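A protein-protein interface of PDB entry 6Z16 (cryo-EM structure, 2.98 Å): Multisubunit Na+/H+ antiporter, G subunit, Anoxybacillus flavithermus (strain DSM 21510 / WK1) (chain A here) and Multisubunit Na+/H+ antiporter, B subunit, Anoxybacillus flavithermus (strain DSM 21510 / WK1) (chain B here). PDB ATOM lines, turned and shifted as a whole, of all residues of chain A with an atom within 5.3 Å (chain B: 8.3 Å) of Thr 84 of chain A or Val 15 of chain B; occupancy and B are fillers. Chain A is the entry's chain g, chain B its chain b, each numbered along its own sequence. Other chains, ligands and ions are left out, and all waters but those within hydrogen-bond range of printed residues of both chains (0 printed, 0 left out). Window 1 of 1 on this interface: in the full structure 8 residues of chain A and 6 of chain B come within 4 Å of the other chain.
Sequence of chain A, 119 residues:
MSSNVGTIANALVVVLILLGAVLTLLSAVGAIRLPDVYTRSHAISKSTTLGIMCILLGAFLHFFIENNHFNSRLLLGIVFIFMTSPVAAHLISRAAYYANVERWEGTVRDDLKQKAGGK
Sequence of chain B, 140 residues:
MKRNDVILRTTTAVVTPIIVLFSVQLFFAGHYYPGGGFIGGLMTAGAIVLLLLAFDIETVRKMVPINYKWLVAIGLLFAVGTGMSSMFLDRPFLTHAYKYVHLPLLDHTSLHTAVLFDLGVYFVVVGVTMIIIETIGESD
O of Phe 80 of chain A is in hydrogen-bond range of OG1 of Thr 84 of chain A (2.5 Å).
Among the printed residues, pairs that only touch across the chains: Phe 80 of chain A with Val 15 of chain B (3.5 Å) and Thr 84 of chain A with Val 15 of chain B (3.8 Å).
Of the printed residues of chain B, Phe 80 of chain A touches Val 15.
Of chain B, only Val 15 comes within 4 Å of Thr 84 of chain A.
Ala 13 of chain B touches none of the printed residues of chain A.
Of the printed residues of chain A, Val 15 of chain B touches Phe 80 and Thr 84.
Hydrophobic or aromatic side chains of chain A within 4 Å of the printed part of chain B: Phe 80.
Among the printed residues, 2 pairs touch across the chains.
Among the printed residues, no Asp or Glu carboxylate lies within 4 Å of a Lys or Arg side-chain nitrogen of the other chain.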
ATOM      1  N   VAL A  79     -22.862  -8.013 -25.969  1.00  0.00           N
ATOM      2  CA  VAL A  79     -24.019  -7.217 -26.383  1.00  0.00           C
ATOM      3  C   VAL A  79     -23.884  -5.771 -25.906  1.00  0.00           C
ATOM      4  O   VAL A  79     -24.192  -4.826 -26.650  1.00  0.00           O
ATOM      5  CB  VAL A  79     -25.316  -7.878 -25.879  1.00  0.00           C
ATOM      6  CG1 VAL A  79     -26.534  -7.011 -26.170  1.00  0.00           C
ATOM      7  CG2 VAL A  79     -25.492  -9.240 -26.523  1.00  0.00           C
ATOM      8  N   PHE A  80     -23.333  -5.571 -24.704  1.00  0.00           N
ATOM      9  CA  PHE A  80     -23.173  -4.221 -24.178  1.00  0.00           C
ATOM     10  C   PHE A  80     -22.130  -3.424 -24.956  1.00  0.00           C
ATOM     11  O   PHE A  80     -22.352  -2.245 -25.257  1.00  0.00           O
ATOM     12  CB  PHE A  80     -22.794  -4.263 -22.698  1.00  0.00           C
ATOM     13  CG  PHE A  80     -22.715  -2.905 -22.077  1.00  0.00           C
ATOM     14  CD1 PHE A  80     -23.866  -2.246 -21.704  1.00  0.00           C
ATOM     15  CD2 PHE A  80     -21.496  -2.263 -21.918  1.00  0.00           C
ATOM     16  CE1 PHE A  80     -23.806  -0.994 -21.158  1.00  0.00           C
ATOM     17  CE2 PHE A  80     -21.437  -0.997 -21.391  1.00  0.00           C
ATOM     18  CZ  PHE A  80     -22.596  -0.364 -21.002  1.00  0.00           C
ATOM     19  N   ILE A  81     -20.978  -4.034 -25.252  1.00  0.00           N
ATOM     20  CA  ILE A  81     -19.921  -3.319 -25.965  1.00  0.00           C
ATOM     21  C   ILE A  81     -20.364  -2.992 -27.384  1.00  0.00           C
ATOM     22  O   ILE A  81     -20.134  -1.873 -27.873  1.00  0.00           O
ATOM     23  CB  ILE A  81     -18.611  -4.129 -25.947  1.00  0.00           C
ATOM     24  CG1 ILE A  81     -18.087  -4.288 -24.521  1.00  0.00           C
ATOM     25  CG2 ILE A  81     -17.558  -3.446 -26.771  1.00  0.00           C
ATOM     26  CD1 ILE A  81     -17.780  -2.985 -23.830  1.00  0.00           C
ATOM     27  N   PHE A  82     -21.054  -3.941 -28.037  1.00  0.00           N
ATOM     28  CA  PHE A  82     -21.644  -3.698 -29.351  1.00  0.00           C
ATOM     29  C   PHE A  82     -22.644  -2.550 -29.316  1.00  0.00           C
ATOM     30  O   PHE A  82     -22.718  -1.754 -30.258  1.00  0.00           O
ATOM     31  CB  PHE A  82     -22.326  -4.971 -29.843  1.00  0.00           C
ATOM     32  CG  PHE A  82     -22.900  -4.864 -31.225  1.00  0.00           C
ATOM     33  CD1 PHE A  82     -22.082  -4.970 -32.335  1.00  0.00           C
ATOM     34  CD2 PHE A  82     -24.261  -4.668 -31.416  1.00  0.00           C
ATOM     35  CE1 PHE A  82     -22.605  -4.883 -33.609  1.00  0.00           C
ATOM     36  CE2 PHE A  82     -24.789  -4.574 -32.687  1.00  0.00           C
ATOM     37  CZ  PHE A  82     -23.959  -4.683 -33.785  1.00  0.00           C
ATOM     38  N   MET A  83     -23.409  -2.436 -28.230  1.00  0.00           N
ATOM     39  CA  MET A  83     -24.375  -1.351 -28.135  1.00  0.00           C
ATOM     40  C   MET A  83     -23.708  -0.010 -27.841  1.00  0.00           C
ATOM     41  O   MET A  83     -24.191   1.031 -28.299  1.00  0.00           O
ATOM     42  CB  MET A  83     -25.407  -1.685 -27.056  1.00  0.00           C
ATOM     43  CG  MET A  83     -26.599  -0.750 -26.981  1.00  0.00           C
ATOM     44  SD  MET A  83     -27.594  -0.802 -28.477  1.00  0.00           S
ATOM     45  CE  MET A  83     -28.330  -2.428 -28.345  1.00  0.00           C
ATOM     46  N   THR A  84     -22.593  -0.005 -27.105  1.00  0.00           N
ATOM     47  CA  THR A  84     -22.135   1.225 -26.473  1.00  0.00           C
ATOM     48  C   THR A  84     -20.860   1.846 -27.029  1.00  0.00           C
ATOM     49  O   THR A  84     -20.658   3.046 -26.828  1.00  0.00           O
ATOM     50  CB  THR A  84     -21.942   0.997 -24.970  1.00  0.00           C
ATOM     51  OG1 THR A  84     -21.087  -0.132 -24.761  1.00  0.00           O
ATOM     52  CG2 THR A  84     -23.278   0.773 -24.309  1.00  0.00           C
ATOM     53  N   SER A  85     -19.985   1.095 -27.691  1.00  0.00           N
ATOM     54  CA  SER A  85     -18.789   1.794 -28.173  1.00  0.00           C
ATOM     55  C   SER A  85     -18.983   2.688 -29.415  1.00  0.00           C
ATOM     56  O   SER A  85     -18.363   3.768 -29.455  1.00  0.00           O
ATOM     57  CB  SER A  85     -17.637   0.798 -28.374  1.00  0.00           C
ATOM     58  OG  SER A  85     -17.898  -0.197 -29.335  1.00  0.00           O
ATOM     59  N   PRO A  86     -19.807   2.350 -30.430  1.00  0.00           N
ATOM     60  CA  PRO A  86     -19.999   3.328 -31.512  1.00  0.00           C
ATOM     61  C   PRO A  86     -20.795   4.554 -31.107  1.00  0.00           C
ATOM     62  O   PRO A  86     -20.578   5.622 -31.689  1.00  0.00           O
ATOM     63  CB  PRO A  86     -20.730   2.526 -32.593  1.00  0.00           C
ATOM     64  CG  PRO A  86     -20.411   1.151 -32.316  1.00  0.00           C
ATOM     65  CD  PRO A  86     -20.390   1.059 -30.845  1.00  0.00           C
ATOM     66  N   VAL A  87     -21.688   4.459 -30.121  1.00  0.00           N
ATOM     67  CA  VAL A  87     -22.372   5.671 -29.679  1.00  0.00           C
ATOM     68  C   VAL A  87     -21.422   6.533 -28.849  1.00  0.00           C
ATOM     69  O   VAL A  87     -21.534   7.768 -28.841  1.00  0.00           O
ATOM     70  CB  VAL A  87     -23.682   5.320 -28.937  1.00  0.00           C
ATOM     71  CG1 VAL A  87     -23.426   4.582 -27.646  1.00  0.00           C
ATOM     72  CG2 VAL A  87     -24.522   6.561 -28.681  1.00  0.00           C
ATOM     73  N   ALA A  88     -20.426   5.912 -28.210  1.00  0.00           N
ATOM     74  CA  ALA A  88     -19.366   6.673 -27.559  1.00  0.00           C
ATOM     75  C   ALA A  88     -18.545   7.447 -28.583  1.00  0.00           C
ATOM     76  O   ALA A  88     -18.272   8.640 -28.401  1.00  0.00           O
ATOM     77  CB  ALA A  88     -18.474   5.737 -26.747  1.00  0.00           C
ATOM     78  N   LEU B   8     -28.535   9.394 -27.573  1.00  0.00           N
ATOM     79  CA  LEU B   8     -28.103   9.210 -26.191  1.00  0.00           C
ATOM     80  C   LEU B   8     -29.253   8.777 -25.294  1.00  0.00           C
ATOM     81  O   LEU B   8     -29.087   7.870 -24.472  1.00  0.00           O
ATOM     82  CB  LEU B   8     -27.477  10.497 -25.663  1.00  0.00           C
ATOM     83  CG  LEU B   8     -26.994  10.443 -24.213  1.00  0.00           C
ATOM     84  CD1 LEU B   8     -25.934   9.374 -24.031  1.00  0.00           C
ATOM     85  CD2 LEU B   8     -26.472  11.793 -23.783  1.00  0.00           C
ATOM     86  N   ARG B   9     -30.431   9.394 -25.449  1.00  0.00           N
ATOM     87  CA  ARG B   9     -31.574   9.018 -24.622  1.00  0.00           C
ATOM     88  C   ARG B   9     -32.059   7.610 -24.935  1.00  0.00           C
ATOM     89  O   ARG B   9     -32.419   6.859 -24.022  1.00  0.00           O
ATOM     90  CB  ARG B   9     -32.714  10.023 -24.781  1.00  0.00           C
ATOM     91  CG  ARG B   9     -32.463  11.349 -24.088  1.00  0.00           C
ATOM     92  CD  ARG B   9     -33.694  12.243 -24.092  1.00  0.00           C
ATOM     93  NE  ARG B   9     -34.013  12.754 -25.418  1.00  0.00           N
ATOM     94  CZ  ARG B   9     -35.101  12.425 -26.105  1.00  0.00           C
ATOM     95  NH1 ARG B   9     -35.981  11.577 -25.592  1.00  0.00           N
ATOM     96  NH2 ARG B   9     -35.310  12.943 -27.305  1.00  0.00           N
ATOM     97  N   THR B  10     -32.038   7.209 -26.208  1.00  0.00           N
ATOM     98  CA  THR B  10     -32.539   5.874 -26.510  1.00  0.00           C
ATOM     99  C   THR B  10     -31.541   4.794 -26.104  1.00  0.00           C
ATOM    100  O   THR B  10     -31.941   3.739 -25.583  1.00  0.00           O
ATOM    101  CB  THR B  10     -32.890   5.762 -27.986  1.00  0.00           C
ATOM    102  OG1 THR B  10     -33.728   6.864 -28.349  1.00  0.00           O
ATOM    103  CG2 THR B  10     -33.682   4.495 -28.221  1.00  0.00           C
ATOM    104  N   THR B  11     -30.236   5.043 -26.283  1.00  0.00           N
ATOM    105  CA  THR B  11     -29.284   4.061 -25.785  1.00  0.00           C
ATOM    106  C   THR B  11     -29.224   4.054 -24.262  1.00  0.00           C
ATOM    107  O   THR B  11     -28.956   3.003 -23.682  1.00  0.00           O
ATOM    108  CB  THR B  11     -27.890   4.266 -26.397  1.00  0.00           C
ATOM    109  OG1 THR B  11     -27.078   3.124 -26.102  1.00  0.00           O
ATOM    110  CG2 THR B  11     -27.189   5.487 -25.841  1.00  0.00           C
ATOM    111  N   THR B  12     -29.572   5.163 -23.597  1.00  0.00           N
ATOM    112  CA  THR B  12     -29.700   5.144 -22.145  1.00  0.00           C
ATOM    113  C   THR B  12     -30.892   4.302 -21.719  1.00  0.00           C
ATOM    114  O   THR B  12     -30.793   3.511 -20.772  1.00  0.00           O
ATOM    115  CB  THR B  12     -29.826   6.572 -21.622  1.00  0.00           C
ATOM    116  OG1 THR B  12     -28.671   7.321 -22.017  1.00  0.00           O
ATOM    117  CG2 THR B  12     -29.933   6.593 -20.113  1.00  0.00           C
ATOM    118  N   ALA B  13     -32.008   4.427 -22.446  1.00  0.00           N
ATOM    119  CA  ALA B  13     -33.203   3.646 -22.146  1.00  0.00           C
ATOM    120  C   ALA B  13     -32.983   2.153 -22.345  1.00  0.00           C
ATOM    121  O   ALA B  13     -33.558   1.347 -21.610  1.00  0.00           O
ATOM    122  CB  ALA B  13     -34.369   4.120 -23.011  1.00  0.00           C
ATOM    123  N   VAL B  14     -32.162   1.755 -23.320  1.00  0.00           N
ATOM    124  CA  VAL B  14     -31.910   0.322 -23.492  1.00  0.00           C
ATOM    125  C   VAL B  14     -30.670  -0.176 -22.759  1.00  0.00           C
ATOM    126  O   VAL B  14     -30.430  -1.392 -22.737  1.00  0.00           O
ATOM    127  CB  VAL B  14     -31.770  -0.081 -24.972  1.00  0.00           C
ATOM    128  CG1 VAL B  14     -33.024   0.273 -25.739  1.00  0.00           C
ATOM    129  CG2 VAL B  14     -30.556   0.562 -25.583  1.00  0.00           C
ATOM    130  N   VAL B  15     -29.873   0.710 -22.167  1.00  0.00           N
ATOM    131  CA  VAL B  15     -28.652   0.311 -21.472  1.00  0.00           C
ATOM    132  C   VAL B  15     -28.857   0.274 -19.956  1.00  0.00           C
ATOM    133  O   VAL B  15     -28.284  -0.582 -19.270  1.00  0.00           O
ATOM    134  CB  VAL B  15     -27.495   1.234 -21.925  1.00  0.00           C
ATOM    135  CG1 VAL B  15     -26.408   1.371 -20.906  1.00  0.00           C
ATOM    136  CG2 VAL B  15     -26.849   0.637 -23.168  1.00  0.00           C
ATOM    137  N   THR B  16     -29.727   1.144 -19.436  1.00  0.00           N
ATOM    138  CA  THR B  16     -30.028   1.153 -18.003  1.00  0.00           C
ATOM    139  C   THR B  16     -30.594  -0.164 -17.430  1.00  0.00           C
ATOM    140  O   THR B  16     -30.140  -0.553 -16.334  1.00  0.00           O
ATOM    141  CB  THR B  16     -30.948   2.352 -17.711  1.00  0.00           C
ATOM    142  OG1 THR B  16     -30.311   3.557 -18.151  1.00  0.00           O
ATOM    143  CG2 THR B  16     -31.245   2.475 -16.237  1.00  0.00           C
ATOM    144  N   PRO B  17     -31.515  -0.908 -18.087  1.00  0.00           N
ATOM    145  CA  PRO B  17     -31.940  -2.192 -17.500  1.00  0.00           C
ATOM    146  C   PRO B  17     -30.851  -3.238 -17.365  1.00  0.00           C
ATOM    147  O   PRO B  17     -30.878  -3.996 -16.390  1.00  0.00           O
ATOM    148  CB  PRO B  17     -33.033  -2.675 -18.460  1.00  0.00           C
ATOM    149  CG  PRO B  17     -33.558  -1.482 -19.038  1.00  0.00           C
ATOM    150  CD  PRO B  17     -32.410  -0.574 -19.215  1.00  0.00           C
ATOM    151  N   ILE B  18     -29.880  -3.299 -18.272  1.00  0.00           N
ATOM    152  CA  ILE B  18     -28.876  -4.345 -18.100  1.00  0.00           C
ATOM    153  C   ILE B  18     -27.869  -3.955 -17.016  1.00  0.00           C
ATOM    154  O   ILE B  18     -27.331  -4.829 -16.327  1.00  0.00           O
ATOM    155  CB  ILE B  18     -28.218  -4.705 -19.448  1.00  0.00           C
ATOM    156  CG1 ILE B  18     -27.440  -6.015 -19.323  1.00  0.00           C
ATOM    157  CG2 ILE B  18     -27.298  -3.619 -19.952  1.00  0.00           C
ATOM    158  CD1 ILE B  18     -28.298  -7.177 -18.910  1.00  0.00           C
ATOM    159  N   ILE B  19     -27.679  -2.653 -16.773  1.00  0.00           N
ATOM    160  CA  ILE B  19     -26.879  -2.221 -15.629  1.00  0.00           C
ATOM    161  C   ILE B  19     -27.589  -2.564 -14.326  1.00  0.00           C
ATOM    162  O   ILE B  19     -26.956  -3.020 -13.365  1.00  0.00           O
ATOM    163  CB  ILE B  19     -26.573  -0.713 -15.714  1.00  0.00           C
ATOM    164  CG1 ILE B  19     -25.831  -0.372 -16.998  1.00  0.00           C
ATOM    165  CG2 ILE B  19     -25.700  -0.282 -14.554  1.00  0.00           C
ATOM    166  CD1 ILE B  19     -25.668   1.105 -17.207  1.00  0.00           C
ATOM    167  N   VAL B  20     -28.913  -2.384 -14.280  1.00  0.00           N
ATOM    168  CA  VAL B  20     -29.650  -2.686 -13.054  1.00  0.00           C
ATOM    169  C   VAL B  20     -29.684  -4.192 -12.788  1.00  0.00           C
ATOM    170  O   VAL B  20     -29.489  -4.629 -11.644  1.00  0.00           O
ATOM    171  CB  VAL B  20     -31.061  -2.071 -13.113  1.00  0.00           C
ATOM    172  CG1 VAL B  20     -31.875  -2.474 -11.909  1.00  0.00           C
ATOM    173  CG2 VAL B  20     -30.965  -0.565 -13.152  1.00  0.00           C
ATOM    174  N   LEU B  21     -29.891  -5.008 -13.834  1.00  0.00           N
ATOM    175  CA  LEU B  21     -29.796  -6.462 -13.677  1.00  0.00           C
ATOM    176  C   LEU B  21     -28.401  -6.896 -13.256  1.00  0.00           C
ATOM    177  O   LEU B  21     -28.256  -7.822 -12.455  1.00  0.00           O
ATOM    178  CB  LEU B  21     -30.174  -7.208 -14.957  1.00  0.00           C
ATOM    179  CG  LEU B  21     -31.581  -7.745 -15.237  1.00  0.00           C
ATOM    180  CD1 LEU B  21     -32.528  -6.711 -15.746  1.00  0.00           C
ATOM    181  CD2 LEU B  21     -31.503  -8.897 -16.208  1.00  0.00           C
ATOM    182  N   PHE B  22     -27.367  -6.226 -13.767  1.00  0.00           N
ATOM    183  CA  PHE B  22     -26.006  -6.582 -13.388  1.00  0.00           C
ATOM    184  C   PHE B  22     -25.725  -6.238 -11.930  1.00  0.00           C
ATOM    185  O   PHE B  22     -25.084  -7.021 -11.221  1.00  0.00           O
ATOM    186  CB  PHE B  22     -25.018  -5.893 -14.327  1.00  0.00           C
ATOM    187  CG  PHE B  22     -23.585  -6.174 -14.007  1.00  0.00           C
ATOM    188  CD1 PHE B  22     -23.079  -7.459 -14.115  1.00  0.00           C
ATOM    189  CD2 PHE B  22     -22.733  -5.148 -13.642  1.00  0.00           C
ATOM    190  CE1 PHE B  22     -21.756  -7.722 -13.833  1.00  0.00           C
ATOM    191  CE2 PHE B  22     -21.409  -5.401 -13.365  1.00  0.00           C
ATOM    192  CZ  PHE B  22     -20.920  -6.690 -13.458  1.00  0.00           C
ATOM    193  N   GLY B  46     -24.504   3.871 -10.317  1.00  0.00           N
ATOM    194  CA  GLY B  46     -24.011   4.171 -11.655  1.00  0.00           C
ATOM    195  C   GLY B  46     -25.102   4.208 -12.712  1.00  0.00           C
ATOM    196  O   GLY B  46     -25.052   5.025 -13.638  1.00  0.00           O
ATOM    197  N   ALA B  47     -26.094   3.321 -12.595  1.00  0.00           N
ATOM    198  CA  ALA B  47     -27.258   3.384 -13.476  1.00  0.00           C
ATOM    199  C   ALA B  47     -28.033   4.681 -13.273  1.00  0.00           C
ATOM    200  O   ALA B  47     -28.463   5.324 -14.245  1.00  0.00           O
ATOM    201  CB  ALA B  47     -28.168   2.184 -13.234  1.00  0.00           C
ATOM    202  N   LEU B  50     -26.111   7.402 -14.958  1.00  0.00           N
ATOM    203  CA  LEU B  50     -26.359   7.431 -16.396  1.00  0.00           C
ATOM    204  C   LEU B  50     -27.683   8.117 -16.715  1.00  0.00           C
ATOM    205  O   LEU B  50     -27.780   8.892 -17.679  1.00  0.00           O
ATOM    206  CB  LEU B  50     -26.335   6.012 -16.949  1.00  0.00           C
ATOM    207  CG  LEU B  50     -26.558   5.887 -18.451  1.00  0.00           C
ATOM    208  CD1 LEU B  50     -25.483   6.609 -19.231  1.00  0.00           C
ATOM    209  CD2 LEU B  50     -26.586   4.434 -18.823  1.00  0.00           C
ATOM    210  N   LEU B  51     -28.703   7.871 -15.887  1.00  0.00           N
ATOM    211  CA  LEU B  51     -29.958   8.610 -16.013  1.00  0.00           C
ATOM    212  C   LEU B  51     -29.779  10.103 -15.749  1.00  0.00           C
ATOM    213  O   LEU B  51     -30.462  10.926 -16.367  1.00  0.00           O
ATOM    214  CB  LEU B  51     -31.000   8.028 -15.062  1.00  0.00           C
ATOM    215  CG  LEU B  51     -31.504   6.626 -15.385  1.00  0.00           C
ATOM    216  CD1 LEU B  51     -32.333   6.098 -14.243  1.00  0.00           C
ATOM    217  CD2 LEU B  51     -32.328   6.659 -16.651  1.00  0.00           C
